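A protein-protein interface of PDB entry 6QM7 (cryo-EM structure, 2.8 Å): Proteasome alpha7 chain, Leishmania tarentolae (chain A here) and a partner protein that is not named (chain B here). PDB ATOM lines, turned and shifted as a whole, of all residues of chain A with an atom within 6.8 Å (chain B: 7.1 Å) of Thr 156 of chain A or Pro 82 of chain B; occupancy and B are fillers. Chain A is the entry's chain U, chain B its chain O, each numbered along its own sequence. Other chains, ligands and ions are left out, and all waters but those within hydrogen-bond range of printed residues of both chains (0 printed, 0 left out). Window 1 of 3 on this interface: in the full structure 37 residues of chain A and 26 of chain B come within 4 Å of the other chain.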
ATOM      1  N   GLY A 117      27.691  -6.817  -8.358  1.00  0.00           N
ATOM      2  CA  GLY A 117      27.456  -8.272  -8.357  1.00  0.00           C
ATOM      3  C   GLY A 117      26.138  -8.639  -7.710  1.00  0.00           C
ATOM      4  O   GLY A 117      25.476  -9.525  -8.224  1.00  0.00           O
ATOM      5  N   GLU A 118      25.791  -8.012  -6.591  1.00  0.00           N
ATOM      6  CA  GLU A 118      24.530  -8.280  -5.860  1.00  0.00           C
ATOM      7  C   GLU A 118      23.369  -7.983  -6.800  1.00  0.00           C
ATOM      8  O   GLU A 118      22.414  -8.773  -6.827  1.00  0.00           O
ATOM      9  CB  GLU A 118      24.402  -7.408  -4.612  1.00  0.00           C
ATOM     10  CG  GLU A 118      25.171  -7.914  -3.392  1.00  0.00           C
ATOM     11  CD  GLU A 118      25.419  -6.845  -2.319  1.00  0.00           C
ATOM     12  OE1 GLU A 118      24.534  -5.955  -2.131  1.00  0.00           O
ATOM     13  OE2 GLU A 118      26.497  -6.887  -1.660  1.00  0.00           O
ATOM     14  N   MET A 120      23.439  -7.689 -10.268  1.00  0.00           N
ATOM     15  CA  MET A 120      23.475  -8.636 -11.404  1.00  0.00           C
ATOM     16  C   MET A 120      22.957 -10.017 -10.989  1.00  0.00           C
ATOM     17  O   MET A 120      22.320 -10.670 -11.813  1.00  0.00           O
ATOM     18  CB  MET A 120      24.895  -8.754 -11.943  1.00  0.00           C
ATOM     19  CG  MET A 120      25.270  -7.511 -12.672  1.00  0.00           C
ATOM     20  SD  MET A 120      26.915  -7.557 -13.366  1.00  0.00           S
ATOM     21  CE  MET A 120      26.545  -8.615 -14.759  1.00  0.00           C
ATOM     22  N   HIS A 121      23.240 -10.439  -9.768  1.00  0.00           N
ATOM     23  CA  HIS A 121      22.807 -11.736  -9.206  1.00  0.00           C
ATOM     24  C   HIS A 121      21.297 -11.739  -8.994  1.00  0.00           C
ATOM     25  O   HIS A 121      20.665 -12.743  -9.313  1.00  0.00           O
ATOM     26  CB  HIS A 121      23.523 -12.024  -7.886  1.00  0.00           C
ATOM     27  CG  HIS A 121      22.919 -13.171  -7.164  1.00  0.00           C
ATOM     28  ND1 HIS A 121      22.013 -12.977  -6.141  1.00  0.00           N
ATOM     29  CD2 HIS A 121      23.043 -14.507  -7.349  1.00  0.00           C
ATOM     30  CE1 HIS A 121      21.616 -14.154  -5.708  1.00  0.00           C
ATOM     31  NE2 HIS A 121      22.235 -15.109  -6.434  1.00  0.00           N
ATOM     32  N   THR A 124      19.187 -13.180 -11.511  1.00  0.00           N
ATOM     33  CA  THR A 124      19.407 -14.624 -11.781  1.00  0.00           C
ATOM     34  C   THR A 124      18.527 -15.507 -10.901  1.00  0.00           C
ATOM     35  O   THR A 124      18.617 -16.713 -11.060  1.00  0.00           O
ATOM     36  CB  THR A 124      20.869 -15.008 -11.563  1.00  0.00           C
ATOM     37  OG1 THR A 124      21.233 -15.030 -10.186  1.00  0.00           O
ATOM     38  CG2 THR A 124      21.797 -14.055 -12.273  1.00  0.00           C
ATOM     39  N   VAL A 150      35.525  -7.748 -11.788  1.00  0.00           N
ATOM     40  CA  VAL A 150      34.657  -8.192 -12.904  1.00  0.00           C
ATOM     41  C   VAL A 150      33.463  -8.890 -12.286  1.00  0.00           C
ATOM     42  O   VAL A 150      33.660  -9.981 -11.747  1.00  0.00           O
ATOM     43  CB  VAL A 150      35.400  -9.127 -13.869  1.00  0.00           C
ATOM     44  CG1 VAL A 150      34.441  -9.670 -14.916  1.00  0.00           C
ATOM     45  CG2 VAL A 150      36.591  -8.434 -14.505  1.00  0.00           C
ATOM     46  N   SER A 151      32.300  -8.248 -12.328  1.00  0.00           N
ATOM     47  CA  SER A 151      30.981  -8.896 -12.145  1.00  0.00           C
ATOM     48  C   SER A 151      30.578  -9.503 -13.484  1.00  0.00           C
ATOM     49  O   SER A 151      30.635  -8.772 -14.475  1.00  0.00           O
ATOM     50  CB  SER A 151      29.953  -7.922 -11.676  1.00  0.00           C
ATOM     51  OG  SER A 151      28.733  -8.588 -11.395  1.00  0.00           O
ATOM     52  N   ASP A 152      30.231 -10.788 -13.502  1.00  0.00           N
ATOM     53  CA  ASP A 152      29.735 -11.504 -14.705  1.00  0.00           C
ATOM     54  C   ASP A 152      28.219 -11.627 -14.577  1.00  0.00           C
ATOM     55  O   ASP A 152      27.659 -11.224 -13.560  1.00  0.00           O
ATOM     56  CB  ASP A 152      30.481 -12.830 -14.885  1.00  0.00           C
ATOM     57  CG  ASP A 152      29.854 -13.990 -14.132  1.00  0.00           C
ATOM     58  OD1 ASP A 152      29.090 -14.770 -14.752  1.00  0.00           O
ATOM     59  OD2 ASP A 152      30.126 -14.097 -12.926  1.00  0.00           O
ATOM     60  N   PRO A 153      27.501 -12.156 -15.598  1.00  0.00           N
ATOM     61  CA  PRO A 153      26.037 -12.242 -15.560  1.00  0.00           C
ATOM     62  C   PRO A 153      25.430 -12.954 -14.341  1.00  0.00           C
ATOM     63  O   PRO A 153      24.341 -12.572 -13.944  1.00  0.00           O
ATOM     64  CB  PRO A 153      25.740 -13.069 -16.816  1.00  0.00           C
ATOM     65  CG  PRO A 153      26.822 -12.647 -17.763  1.00  0.00           C
ATOM     66  CD  PRO A 153      28.044 -12.653 -16.875  1.00  0.00           C
ATOM     67  N   SER A 154      26.153 -13.950 -13.819  1.00  0.00           N
ATOM     68  CA  SER A 154      25.814 -14.761 -12.623  1.00  0.00           C
ATOM     69  C   SER A 154      25.772 -13.909 -11.353  1.00  0.00           C
ATOM     70  O   SER A 154      25.113 -14.358 -10.391  1.00  0.00           O
ATOM     71  CB  SER A 154      26.800 -15.882 -12.436  1.00  0.00           C
ATOM     72  OG  SER A 154      28.056 -15.373 -12.037  1.00  0.00           O
ATOM     73  N   GLY A 155      26.476 -12.776 -11.339  1.00  0.00           N
ATOM     74  CA  GLY A 155      26.683 -11.943 -10.146  1.00  0.00           C
ATOM     75  C   GLY A 155      28.031 -12.202  -9.492  1.00  0.00           C
ATOM     76  O   GLY A 155      28.353 -11.465  -8.553  1.00  0.00           O
ATOM     77  N   THR A 156      28.784 -13.208  -9.952  1.00  0.00           N
ATOM     78  CA  THR A 156      30.108 -13.590  -9.394  1.00  0.00           C
ATOM     79  C   THR A 156      31.090 -12.439  -9.614  1.00  0.00           C
ATOM     80  O   THR A 156      31.438 -12.165 -10.772  1.00  0.00           O
ATOM     81  CB  THR A 156      30.699 -14.857 -10.035  1.00  0.00           C
ATOM     82  OG1 THR A 156      29.748 -15.923 -10.030  1.00  0.00           O
ATOM     83  CG2 THR A 156      31.948 -15.334  -9.326  1.00  0.00           C
ATOM     84  N   VAL A 157      31.509 -11.802  -8.528  1.00  0.00           N
ATOM     85  CA  VAL A 157      32.566 -10.753  -8.510  1.00  0.00           C
ATOM     86  C   VAL A 157      33.894 -11.443  -8.219  1.00  0.00           C
ATOM     87  O   VAL A 157      33.903 -12.390  -7.419  1.00  0.00           O
ATOM     88  CB  VAL A 157      32.261  -9.694  -7.441  1.00  0.00           C
ATOM     89  CG1 VAL A 157      33.286  -8.577  -7.428  1.00  0.00           C
ATOM     90  CG2 VAL A 157      30.865  -9.139  -7.610  1.00  0.00           C
ATOM     91  N   ALA A 158      34.964 -10.978  -8.848  1.00  0.00           N
ATOM     92  CA  ALA A 158      36.346 -11.384  -8.525  1.00  0.00           C
ATOM     93  C   ALA A 158      37.286 -10.227  -8.823  1.00  0.00           C
ATOM     94  O   ALA A 158      37.082  -9.542  -9.831  1.00  0.00           O
ATOM     95  CB  ALA A 158      36.716 -12.600  -9.313  1.00  0.00           C
ATOM     96  N   VAL B  63      38.672 -12.891  -3.805  1.00  0.00           N
ATOM     97  CA  VAL B  63      37.775 -14.078  -3.789  1.00  0.00           C
ATOM     98  C   VAL B  63      37.844 -14.703  -2.397  1.00  0.00           C
ATOM     99  O   VAL B  63      38.900 -15.257  -2.054  1.00  0.00           O
ATOM    100  CB  VAL B  63      38.157 -15.088  -4.884  1.00  0.00           C
ATOM    101  CG1 VAL B  63      37.303 -16.352  -4.809  1.00  0.00           C
ATOM    102  CG2 VAL B  63      38.074 -14.442  -6.262  1.00  0.00           C
ATOM    103  N   TYR B  67      32.871 -14.749   5.053  1.00  0.00           N
ATOM    104  CA  TYR B  67      32.342 -13.388   5.271  1.00  0.00           C
ATOM    105  C   TYR B  67      32.119 -13.215   6.765  1.00  0.00           C
ATOM    106  O   TYR B  67      31.855 -14.201   7.434  1.00  0.00           O
ATOM    107  CB  TYR B  67      31.048 -13.197   4.481  1.00  0.00           C
ATOM    108  CG  TYR B  67      31.106 -13.530   3.006  1.00  0.00           C
ATOM    109  CD1 TYR B  67      31.390 -12.566   2.051  1.00  0.00           C
ATOM    110  CD2 TYR B  67      30.814 -14.804   2.553  1.00  0.00           C
ATOM    111  CE1 TYR B  67      31.416 -12.866   0.696  1.00  0.00           C
ATOM    112  CE2 TYR B  67      30.817 -15.119   1.203  1.00  0.00           C
ATOM    113  CZ  TYR B  67      31.124 -14.149   0.264  1.00  0.00           C
ATOM    114  OH  TYR B  67      31.137 -14.461  -1.068  1.00  0.00           O
ATOM    115  N   GLY B  79      28.997 -23.284  -2.515  1.00  0.00           N
ATOM    116  CA  GLY B  79      28.043 -23.389  -3.633  1.00  0.00           C
ATOM    117  C   GLY B  79      28.172 -22.205  -4.555  1.00  0.00           C
ATOM    118  O   GLY B  79      29.307 -21.704  -4.676  1.00  0.00           O
ATOM    119  N   ARG B  80      27.081 -21.775  -5.195  1.00  0.00           N
ATOM    120  CA  ARG B  80      27.145 -20.596  -6.088  1.00  0.00           C
ATOM    121  C   ARG B  80      27.655 -19.424  -5.238  1.00  0.00           C
ATOM    122  O   ARG B  80      26.903 -18.950  -4.358  1.00  0.00           O
ATOM    123  CB  ARG B  80      25.811 -20.214  -6.735  1.00  0.00           C
ATOM    124  CG  ARG B  80      25.062 -21.344  -7.423  1.00  0.00           C
ATOM    125  CD  ARG B  80      24.702 -21.095  -8.889  1.00  0.00           C
ATOM    126  NE  ARG B  80      24.294 -19.741  -9.219  1.00  0.00           N
ATOM    127  CZ  ARG B  80      24.347 -19.211 -10.442  1.00  0.00           C
ATOM    128  NH1 ARG B  80      24.791 -19.906 -11.479  1.00  0.00           N
ATOM    129  NH2 ARG B  80      23.965 -17.954 -10.621  1.00  0.00           N
ATOM    130  N   ALA B  81      28.897 -19.004  -5.474  1.00  0.00           N
ATOM    131  CA  ALA B  81      29.521 -17.829  -4.833  1.00  0.00           C
ATOM    132  C   ALA B  81      28.512 -16.689  -4.731  1.00  0.00           C
ATOM    133  O   ALA B  81      28.272 -16.173  -3.636  1.00  0.00           O
ATOM    134  CB  ALA B  81      30.755 -17.409  -5.594  1.00  0.00           C
ATOM    135  N   PRO B  82      27.907 -16.240  -5.853  1.00  0.00           N
ATOM    136  CA  PRO B  82      27.023 -15.078  -5.815  1.00  0.00           C
ATOM    137  C   PRO B  82      25.731 -15.304  -5.019  1.00  0.00           C
ATOM    138  O   PRO B  82      25.217 -14.331  -4.496  1.00  0.00           O
ATOM    139  CB  PRO B  82      26.731 -14.799  -7.288  1.00  0.00           C
ATOM    140  CG  PRO B  82      26.925 -16.131  -7.956  1.00  0.00           C
ATOM    141  CD  PRO B  82      28.087 -16.752  -7.220  1.00  0.00           C
ATOM    142  N   ASP B  83      25.236 -16.546  -4.972  1.00  0.00           N
ATOM    143  CA  ASP B  83      24.109 -16.942  -4.092  1.00  0.00           C
ATOM    144  C   ASP B  83      24.587 -16.855  -2.640  1.00  0.00           C
ATOM    145  O   ASP B  83      23.816 -16.382  -1.787  1.00  0.00           O
ATOM    146  CB  ASP B  83      23.600 -18.359  -4.372  1.00  0.00           C
ATOM    147  CG  ASP B  83      22.823 -18.561  -5.663  1.00  0.00           C
ATOM    148  OD1 ASP B  83      22.772 -17.631  -6.490  1.00  0.00           O
ATOM    149  OD2 ASP B  83      22.278 -19.661  -5.832  1.00  0.00           O
ATOM    150  N   GLY B  84      25.805 -17.320  -2.370  1.00  0.00           N
ATOM    151  CA  GLY B  84      26.428 -17.206  -1.044  1.00  0.00           C
ATOM    152  C   GLY B  84      26.478 -15.758  -0.624  1.00  0.00           C
ATOM    153  O   GLY B  84      25.919 -15.427   0.427  1.00  0.00           O
ATOM    154  N   ARG B  85      27.091 -14.920  -1.456  1.00  0.00           N
ATOM    155  CA  ARG B  85      27.181 -13.452  -1.245  1.00  0.00           C
ATOM    156  C   ARG B  85      25.794 -12.889  -0.918  1.00  0.00           C
ATOM    157  O   ARG B  85      25.709 -12.040  -0.018  1.00  0.00           O
ATOM    158  CB  ARG B  85      27.775 -12.793  -2.490  1.00  0.00           C
ATOM    159  CG  ARG B  85      27.876 -11.278  -2.430  1.00  0.00           C
ATOM    160  CD  ARG B  85      28.964 -10.827  -1.479  1.00  0.00           C
ATOM    161  NE  ARG B  85      28.632  -9.562  -0.843  1.00  0.00           N
ATOM    162  CZ  ARG B  85      29.468  -8.829  -0.109  1.00  0.00           C
ATOM    163  NH1 ARG B  85      30.717  -9.226   0.098  1.00  0.00           N
ATOM    164  NH2 ARG B  85      29.048  -7.685   0.408  1.00  0.00           N
ATOM    165  N   ALA B  86      24.755 -13.350  -1.614  1.00  0.00           N
ATOM    166  CA  ALA B  86      23.359 -12.881  -1.468  1.00  0.00           C
ATOM    167  C   ALA B  86      22.817 -13.215  -0.086  1.00  0.00           C
ATOM    168  O   ALA B  86      22.107 -12.367   0.469  1.00  0.00           O
ATOM    169  CB  ALA B  86      22.484 -13.506  -2.514  1.00  0.00           C
ATOM    170  N   LEU B  87      23.073 -14.433   0.398  1.00  0.00           N
ATOM    171  CA  LEU B  87      22.612 -14.910   1.729  1.00  0.00           C
ATOM    172  C   LEU B  87      23.365 -14.175   2.826  1.00  0.00           C
ATOM    173  O   LEU B  87      22.785 -13.978   3.912  1.00  0.00           O
ATOM    174  CB  LEU B  87      22.866 -16.408   1.885  1.00  0.00           C
ATOM    175  CG  LEU B  87      21.924 -17.340   1.133  1.00  0.00           C
ATOM    176  CD1 LEU B  87      22.062 -18.735   1.703  1.00  0.00           C
ATOM    177  CD2 LEU B  87      20.470 -16.883   1.208  1.00  0.00           C
ATOM    178  N   ARG B 129      14.200 -18.831  -7.036  1.00  0.00           N
ATOM    179  CA  ARG B 129      15.211 -19.905  -7.079  1.00  0.00           C
ATOM    180  C   ARG B 129      15.745 -20.100  -5.668  1.00  0.00           C
ATOM    181  O   ARG B 129      16.009 -19.120  -4.985  1.00  0.00           O
ATOM    182  CB  ARG B 129      16.356 -19.539  -8.021  1.00  0.00           C
ATOM    183  CG  ARG B 129      17.347 -20.674  -8.212  1.00  0.00           C
ATOM    184  CD  ARG B 129      18.242 -20.500  -9.419  1.00  0.00           C
ATOM    185  NE  ARG B 129      18.986 -19.258  -9.514  1.00  0.00           N
ATOM    186  CZ  ARG B 129      20.005 -18.912  -8.741  1.00  0.00           C
ATOM    187  NH1 ARG B 129      20.378 -19.689  -7.740  1.00  0.00           N
ATOM    188  NH2 ARG B 129      20.633 -17.766  -8.938  1.00  0.00           N
ATOM    189  N   MET B 131      18.714 -20.451  -3.065  1.00  0.00           N
ATOM    190  CA  MET B 131      20.151 -20.091  -3.065  1.00  0.00           C
ATOM    191  C   MET B 131      20.926 -21.390  -2.920  1.00  0.00           C
ATOM    192  O   MET B 131      20.789 -22.034  -1.875  1.00  0.00           O
ATOM    193  CB  MET B 131      20.512 -19.108  -1.952  1.00  0.00           C
ATOM    194  CG  MET B 131      19.945 -17.716  -2.179  1.00  0.00           C
ATOM    195  SD  MET B 131      19.931 -17.151  -3.916  1.00  0.00           S
ATOM    196  CE  MET B 131      19.005 -15.635  -3.660  1.00  0.00           C
ATOM    197  N   VAL B 133      23.491 -22.951  -2.031  1.00  0.00           N
ATOM    198  CA  VAL B 133      24.650 -22.690  -1.155  1.00  0.00           C
ATOM    199  C   VAL B 133      24.365 -23.252   0.233  1.00  0.00           C
ATOM    200  O   VAL B 133      23.227 -23.148   0.696  1.00  0.00           O
ATOM    201  CB  VAL B 133      24.952 -21.183  -1.152  1.00  0.00           C
ATOM    202  CG1 VAL B 133      24.046 -20.379  -0.232  1.00  0.00           C
ATOM    203  CG2 VAL B 133      26.404 -20.925  -0.814  1.00  0.00           C
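Pro 82 of chain B touches four residues of chain A. Printed residues of chain B within 4 Å of His 121 of chain A: Pro 82 (3.6 Å), Asp 83 (2.6 Å), Ala 86 (3.4 Å), Arg 129 (3.99 Å) and Met 131 (3.6 Å). Printed residues of chain A within 4 Å of Val 63 of chain B: Ala 158 (3.8 Å). Of the printed residues of chain A, Arg 85 of chain B touches Glu 118 (3.4 Å). Tyr 67 of chain B touches none of the printed residues of chain A. Leu 87 of chain B touches none of the printed residues of chain A. The nearest residue of chain B that does not touch Thr 156 of chain A is Ala 81 of chain B (4.4 Å). The nearest residue of chain A that does not touch Pro 82 of chain B is Gly 117 of chain A (5.5 Å). The nearest printed residue of chain A that does not touch Arg 80 of chain B is Thr 124 of chain A (4.03 Å).
The guanidinium group (NE) of Arg 80 of chain B lies within salt-bridge range of the side-chain carboxylate (OD1) of Asp 83 of chain B. The guanidinium group of Arg 129 of chain B lies within salt-bridge range of the side-chain carboxylate of Asp 83 of chain B (2.7 Å). OG1 of Thr 124 of chain A lies within hydrogen-bond range of O of His 121 of chain A (2.5 Å). N of Val 150 of chain A sits at hydrogen-bond distance from O of Ala 158 of chain A (3.1 Å). The side-chain carboxylate (OD2) of Asp 152 of chain A sits close to the backbone NH (N) of Thr 156 of chain A, at 3.4 Å. OG of Ser 154 of chain A is in hydrogen-bond range of OG1 of Thr 156 of chain A, at 2.7 Å.
Among the printed residues, pairs that only touch across the chains: Thr 156 of chain A with Pro 82 of chain B (3.4 Å), His 121 of chain A with Ala 86 of chain B (3.4 Å), Ser 154 of chain A with Pro 82 of chain B (3.5 Å), His 121 of chain A with Pro 82 of chain B (3.6 Å), His 121 of chain A with Met 131 of chain B (3.6 Å), Gly 155 of chain A with Pro 82 of chain B (3.6 Å), Ser 154 of chain A with Arg 80 of chain B (3.8 Å), Ala 158 of chain A with Val 63 of chain B (3.8 Å) and His 121 of chain A with Arg 129 of chain B (3.99 Å).
Hydrophobic or aromatic side chains of chain A that line the printed part of chain B: His 121 and Ala 158.
OD1 of Asp 83 of chain B is in hydrogen-bond range of NE2 of His 121 of chain A. NH2 of Arg 85 of chain B lies within salt-bridge range of OE2 of Glu 118 of chain A (3.4 Å). NE of Arg 129 of chain B lies within hydrogen-bond range of O of Thr 124 of chain A (3.0 Å).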
